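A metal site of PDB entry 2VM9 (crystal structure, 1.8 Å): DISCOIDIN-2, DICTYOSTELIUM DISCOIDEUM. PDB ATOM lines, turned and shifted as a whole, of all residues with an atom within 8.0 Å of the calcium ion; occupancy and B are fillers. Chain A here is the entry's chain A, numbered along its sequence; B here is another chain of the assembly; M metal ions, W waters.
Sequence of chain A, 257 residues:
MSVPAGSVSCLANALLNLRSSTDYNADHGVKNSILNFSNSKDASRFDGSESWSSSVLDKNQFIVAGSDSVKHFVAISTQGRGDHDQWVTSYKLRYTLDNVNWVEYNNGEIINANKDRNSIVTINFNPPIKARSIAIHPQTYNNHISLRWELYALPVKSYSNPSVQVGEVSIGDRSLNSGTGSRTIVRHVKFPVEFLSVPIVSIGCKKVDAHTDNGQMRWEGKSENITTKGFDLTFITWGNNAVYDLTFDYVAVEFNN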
ATOM      1  N   PHE A  37      18.837 -37.398   2.411  1.00  0.00           N
ATOM      2  CA  PHE A  37      19.537 -36.186   2.015  1.00  0.00           C
ATOM      3  C   PHE A  37      18.564 -35.206   1.404  1.00  0.00           C
ATOM      4  O   PHE A  37      17.781 -35.571   0.524  1.00  0.00           O
ATOM      5  CB  PHE A  37      20.666 -36.461   0.999  1.00  0.00           C
ATOM      6  CG  PHE A  37      21.351 -35.179   0.546  1.00  0.00           C
ATOM      7  CD1 PHE A  37      22.214 -34.489   1.405  1.00  0.00           C
ATOM      8  CD2 PHE A  37      21.096 -34.639  -0.689  1.00  0.00           C
ATOM      9  CE1 PHE A  37      22.797 -33.249   0.992  1.00  0.00           C
ATOM     10  CE2 PHE A  37      21.679 -33.434  -1.106  1.00  0.00           C
ATOM     11  CZ  PHE A  37      22.543 -32.751  -0.284  1.00  0.00           C
ATOM     12  N   SER A  38      18.591 -33.973   1.883  1.00  0.00           N
ATOM     13  CA  SER A  38      17.789 -32.917   1.272  1.00  0.00           C
ATOM     14  C   SER A  38      18.498 -31.603   1.450  1.00  0.00           C
ATOM     15  O   SER A  38      19.182 -31.381   2.465  1.00  0.00           O
ATOM     16  CB  SER A  38      16.401 -32.879   1.892  1.00  0.00           C
ATOM     17  OG  SER A  38      16.504 -32.379   3.209  1.00  0.00           O
ATOM     18  N   ASN A  39      18.351 -30.722   0.479  1.00  0.00           N
ATOM     19  CA  ASN A  39      19.067 -29.449   0.523  1.00  0.00           C
ATOM     20  C   ASN A  39      18.069 -28.295   0.334  1.00  0.00           C
ATOM     21  O   ASN A  39      16.893 -28.432   0.731  1.00  0.00           O
ATOM     22  CB  ASN A  39      20.318 -29.445  -0.371  1.00  0.00           C
ATOM     23  CG  ASN A  39      19.993 -29.759  -1.825  1.00  0.00           C
ATOM     24  OD1 ASN A  39      18.831 -29.651  -2.255  1.00  0.00           O
ATOM     25  ND2 ASN A  39      21.014 -30.125  -2.607  1.00  0.00           N
ATOM     26  N   SER A  40      18.506 -27.175  -0.226  1.00  0.00           N
ATOM     27  CA  SER A  40      17.631 -26.007  -0.271  1.00  0.00           C
ATOM     28  C   SER A  40      16.386 -26.286  -1.111  1.00  0.00           C
ATOM     29  O   SER A  40      16.469 -26.941  -2.170  1.00  0.00           O
ATOM     30  CB  SER A  40      18.358 -24.778  -0.798  1.00  0.00           C
ATOM     31  OG  SER A  40      17.460 -23.672  -0.818  1.00  0.00           O
ATOM     32  N   LYS A  41      15.249 -25.779  -0.640  1.00  0.00           N
ATOM     33  CA  LYS A  41      14.031 -25.826  -1.462  1.00  0.00           C
ATOM     34  C   LYS A  41      13.905 -24.647  -2.434  1.00  0.00           C
ATOM     35  O   LYS A  41      12.973 -24.624  -3.244  1.00  0.00           O
ATOM     36  CB  LYS A  41      12.796 -25.986  -0.579  1.00  0.00           C
ATOM     37  CG  LYS A  41      12.840 -27.248   0.295  1.00  0.00           C
ATOM     38  CD  LYS A  41      12.677 -28.504  -0.539  1.00  0.00           C
ATOM     39  CE  LYS A  41      14.020 -29.115  -0.966  1.00  0.00           C
ATOM     40  NZ  LYS A  41      14.357 -30.241  -0.049  1.00  0.00           N
ATOM     41  N   ASP A  42      14.857 -23.728  -2.396  1.00  0.00           N
ATOM     42  CA  ASP A  42      14.906 -22.590  -3.275  1.00  0.00           C
ATOM     43  C   ASP A  42      14.933 -23.073  -4.734  1.00  0.00           C
ATOM     44  O   ASP A  42      15.943 -23.614  -5.202  1.00  0.00           O
ATOM     45  CB  ASP A  42      16.125 -21.731  -2.972  1.00  0.00           C
ATOM     46  CG  ASP A  42      16.137 -20.424  -3.726  1.00  0.00           C
ATOM     47  OD1 ASP A  42      15.370 -20.268  -4.715  1.00  0.00           O
ATOM     48  OD2 ASP A  42      16.928 -19.545  -3.316  1.00  0.00           O
ATOM     49  N   ALA A  43      13.832 -22.880  -5.455  1.00  0.00           N
ATOM     50  CA  ALA A  43      13.755 -23.365  -6.832  1.00  0.00           C
ATOM     51  C   ALA A  43      14.565 -22.511  -7.829  1.00  0.00           C
ATOM     52  O   ALA A  43      14.736 -22.892  -9.008  1.00  0.00           O
ATOM     53  CB  ALA A  43      12.297 -23.470  -7.257  1.00  0.00           C
ATOM     54  N   SER A  44      15.120 -21.397  -7.350  1.00  0.00           N
ATOM     55  CA  SER A  44      15.851 -20.457  -8.209  1.00  0.00           C
ATOM     56  C   SER A  44      17.332 -20.757  -8.400  1.00  0.00           C
ATOM     57  O   SER A  44      18.036 -20.055  -9.135  1.00  0.00           O
ATOM     58  CB  SER A  44      15.687 -19.024  -7.703  1.00  0.00           C
ATOM     59  OG  SER A  44      16.573 -18.715  -6.633  1.00  0.00           O
ATOM     60  N   ARG A  45      17.835 -21.774  -7.702  1.00  0.00           N
ATOM     61  CA  ARG A  45      19.235 -22.137  -7.825  1.00  0.00           C
ATOM     62  C   ARG A  45      19.362 -23.642  -7.591  1.00  0.00           C
ATOM     63  O   ARG A  45      18.549 -24.238  -6.890  1.00  0.00           O
ATOM     64  CB  ARG A  45      20.091 -21.363  -6.805  1.00  0.00           C
ATOM     65  CG  ARG A  45      19.782 -21.664  -5.329  1.00  0.00           C
ATOM     66  CD  ARG A  45      20.698 -20.833  -4.373  1.00  0.00           C
ATOM     67  NE  ARG A  45      20.220 -20.928  -2.997  1.00  0.00           N
ATOM     68  CZ  ARG A  45      20.650 -21.841  -2.128  1.00  0.00           C
ATOM     69  NH1 ARG A  45      21.590 -22.712  -2.482  1.00  0.00           N
ATOM     70  NH2 ARG A  45      20.154 -21.873  -0.889  1.00  0.00           N
ATOM     71  N   PHE A  46      20.391 -24.224  -8.184  1.00  0.00           N
ATOM     72  CA  PHE A  46      20.618 -25.657  -8.080  1.00  0.00           C
ATOM     73  C   PHE A  46      21.829 -25.884  -7.166  1.00  0.00           C
ATOM     74  O   PHE A  46      22.947 -25.511  -7.510  1.00  0.00           O
ATOM     75  CB  PHE A  46      20.880 -26.243  -9.462  1.00  0.00           C
ATOM     76  CG  PHE A  46      20.989 -27.741  -9.465  1.00  0.00           C
ATOM     77  CD1 PHE A  46      19.904 -28.506  -9.104  1.00  0.00           C
ATOM     78  CD2 PHE A  46      22.188 -28.366  -9.816  1.00  0.00           C
ATOM     79  CE1 PHE A  46      19.986 -29.893  -9.074  1.00  0.00           C
ATOM     80  CE2 PHE A  46      22.271 -29.753  -9.787  1.00  0.00           C
ATOM     81  CZ  PHE A  46      21.182 -30.511  -9.432  1.00  0.00           C
ATOM     82  N   ASP A  47      21.582 -26.485  -6.016  1.00  0.00           N
ATOM     83  CA  ASP A  47      22.640 -26.757  -5.052  1.00  0.00           C
ATOM     84  C   ASP A  47      23.057 -28.247  -5.057  1.00  0.00           C
ATOM     85  O   ASP A  47      23.820 -28.691  -4.184  1.00  0.00           O
ATOM     86  CB  ASP A  47      22.266 -26.283  -3.647  1.00  0.00           C
ATOM     87  CG  ASP A  47      20.930 -26.853  -3.130  1.00  0.00           C
ATOM     88  OD1 ASP A  47      20.141 -27.402  -3.934  1.00  0.00           O
ATOM     89  OD2 ASP A  47      20.661 -26.706  -1.921  1.00  0.00           O
ATOM     90  N   GLY A  48      22.557 -28.987  -6.033  1.00  0.00           N
ATOM     91  CA  GLY A  48      22.871 -30.397  -6.189  1.00  0.00           C
ATOM     92  C   GLY A  48      21.623 -31.250  -6.129  1.00  0.00           C
ATOM     93  O   GLY A  48      20.610 -30.859  -5.537  1.00  0.00           O
ATOM     94  N   SER A  49      21.692 -32.430  -6.770  1.00  0.00           N
ATOM     95  CA  SER A  49      20.590 -33.377  -6.713  1.00  0.00           C
ATOM     96  C   SER A  49      20.512 -33.953  -5.312  1.00  0.00           C
ATOM     97  O   SER A  49      21.549 -34.140  -4.612  1.00  0.00           O
ATOM     98  CB  SER A  49      20.837 -34.514  -7.702  1.00  0.00           C
ATOM     99  OG  SER A  49      22.111 -35.083  -7.514  1.00  0.00           O
ATOM    100  N   GLU A  50      19.298 -34.252  -4.890  1.00  0.00           N
ATOM    101  CA  GLU A  50      19.095 -34.992  -3.645  1.00  0.00           C
ATOM    102  C   GLU A  50      19.240 -36.493  -3.939  1.00  0.00           C
ATOM    103  O   GLU A  50      18.277 -37.287  -3.819  1.00  0.00           O
ATOM    104  CB  GLU A  50      17.722 -34.622  -3.067  1.00  0.00           C
ATOM    105  CG  GLU A  50      17.710 -33.133  -2.645  1.00  0.00           C
ATOM    106  CD  GLU A  50      16.353 -32.677  -2.140  1.00  0.00           C
ATOM    107  OE1 GLU A  50      15.351 -33.311  -2.469  1.00  0.00           O
ATOM    108  OE2 GLU A  50      16.314 -31.665  -1.410  1.00  0.00           O
ATOM    109  N   ARG A  81      15.508 -40.399  -5.713  1.00  0.00           N
ATOM    110  CA  ARG A  81      16.001 -39.016  -5.715  1.00  0.00           C
ATOM    111  C   ARG A  81      14.968 -38.067  -5.132  1.00  0.00           C
ATOM    112  O   ARG A  81      13.783 -38.112  -5.505  1.00  0.00           O
ATOM    113  CB  ARG A  81      16.338 -38.608  -7.160  1.00  0.00           C
ATOM    114  CG  ARG A  81      16.746 -37.159  -7.292  1.00  0.00           C
ATOM    115  CD  ARG A  81      17.338 -36.854  -8.687  1.00  0.00           C
ATOM    116  NE  ARG A  81      17.596 -35.422  -8.759  1.00  0.00           N
ATOM    117  CZ  ARG A  81      18.119 -34.797  -9.803  1.00  0.00           C
ATOM    118  NH1 ARG A  81      18.486 -35.487 -10.893  1.00  0.00           N
ATOM    119  NH2 ARG A  81      18.285 -33.468  -9.734  1.00  0.00           N
ATOM    120  N   ASP A  83      14.427 -34.714  -5.430  1.00  0.00           N
ATOM    121  CA  ASP A  83      14.003 -33.496  -6.136  1.00  0.00           C
ATOM    122  C   ASP A  83      13.545 -33.714  -7.592  1.00  0.00           C
ATOM    123  O   ASP A  83      13.155 -32.754  -8.270  1.00  0.00           O
ATOM    124  CB  ASP A  83      15.113 -32.449  -6.099  1.00  0.00           C
ATOM    125  CG  ASP A  83      16.406 -32.928  -6.758  1.00  0.00           C
ATOM    126  OD1 ASP A  83      16.910 -34.017  -6.414  1.00  0.00           O
ATOM    127  OD2 ASP A  83      16.910 -32.194  -7.611  1.00  0.00           O
ATOM    128  N   ASP B  23      25.601 -28.357   0.884  1.00  0.00           N
ATOM    129  CA  ASP B  23      26.698 -27.621   0.204  1.00  0.00           C
ATOM    130  C   ASP B  23      26.025 -26.605  -0.707  1.00  0.00           C
ATOM    131  O   ASP B  23      25.098 -26.951  -1.449  1.00  0.00           O
ATOM    132  CB  ASP B  23      27.488 -28.541  -0.718  1.00  0.00           C
ATOM    133  CG  ASP B  23      28.388 -29.512   0.029  1.00  0.00           C
ATOM    134  OD1 ASP B  23      28.715 -29.264   1.224  1.00  0.00           O
ATOM    135  OD2 ASP B  23      28.801 -30.506  -0.621  1.00  0.00           O
ATOM    136  N   TYR B  24      26.508 -25.363  -0.707  1.00  0.00           N
ATOM    137  CA  TYR B  24      25.950 -24.392  -1.646  1.00  0.00           C
ATOM    138  C   TYR B  24      25.945 -24.963  -3.070  1.00  0.00           C
ATOM    139  O   TYR B  24      24.989 -24.800  -3.835  1.00  0.00           O
ATOM    140  CB  TYR B  24      26.743 -23.089  -1.597  1.00  0.00           C
ATOM    141  CG  TYR B  24      25.926 -22.008  -2.221  1.00  0.00           C
ATOM    142  CD1 TYR B  24      24.898 -21.397  -1.494  1.00  0.00           C
ATOM    143  CD2 TYR B  24      26.157 -21.596  -3.534  1.00  0.00           C
ATOM    144  CE1 TYR B  24      24.094 -20.398  -2.070  1.00  0.00           C
ATOM    145  CE2 TYR B  24      25.359 -20.601  -4.130  1.00  0.00           C
ATOM    146  CZ  TYR B  24      24.335 -20.032  -3.387  1.00  0.00           C
ATOM    147  OH  TYR B  24      23.557 -19.022  -3.952  1.00  0.00           O
ATOM    148  N   SER B  55      24.400 -24.908   1.975  1.00  0.00           N
ATOM    149  CA  SER B  55      23.361 -24.380   1.104  1.00  0.00           C
ATOM    150  C   SER B  55      22.270 -23.651   1.903  1.00  0.00           C
ATOM    151  O   SER B  55      21.901 -22.499   1.597  1.00  0.00           O
ATOM    152  CB  SER B  55      22.730 -25.470   0.240  1.00  0.00           C
ATOM    153  OG  SER B  55      21.761 -24.854  -0.612  1.00  0.00           O
ATOM    154  N   VAL B  56      21.777 -24.315   2.939  1.00  0.00           N
ATOM    155  CA  VAL B  56      20.759 -23.785   3.850  1.00  0.00           C
ATOM    156  C   VAL B  56      21.444 -23.011   4.973  1.00  0.00           C
ATOM    157  O   VAL B  56      22.468 -23.437   5.490  1.00  0.00           O
ATOM    158  CB  VAL B  56      19.959 -24.965   4.433  1.00  0.00           C
ATOM    159  CG1 VAL B  56      18.993 -24.476   5.545  1.00  0.00           C
ATOM    160  CG2 VAL B  56      19.218 -25.658   3.300  1.00  0.00           C
HETATM  161 CA    CA M   1      17.755 -28.043  -3.929  1.00  0.00          CA
HETATM  162  O   HOH W   1      17.883 -25.312  -4.406  1.00  0.00           O
HETATM  163  O   HOH W   2      16.241 -29.751  -3.615  1.00  0.00           O
HETATM  164  O   HOH W   3      18.509 -29.014  -6.017  1.00  0.00           O
HETATM  165  O   HOH W   4      16.064 -27.524  -5.698  1.00  0.00           O
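The guanidinium group of Arg 45 is in hydrogen-bond range of the side-chain hydroxyl of Ser 40, at 3.2 Å.
The backbone NH (N) of Asp 42 is in hydrogen-bond range of the side-chain hydroxyl (OG) of Ser 40, at 3.0 Å.
The side-chain carboxylate (OD2) of Asp 47 sits at hydrogen-bond distance from the side-chain hydroxyl (OG) of Ser 55 of chain B, at 2.5 Å.
O of Gly 48 sits at hydrogen-bond distance from ND2 of Asn 39 (3.0 Å).
The backbone NH (N) of Asn 39 is in hydrogen-bond range of the side-chain carboxylate (OE2) of Glu 50 (2.9 Å).
NZ of Lys 41 is in hydrogen-bond range of O of Asn 39 (3.2 Å).
The calcium ion is bound by water W2, water W3, O of Ser 40, OD1 of Asp 47, water W4, OD1 of Asn 39 and water W1.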
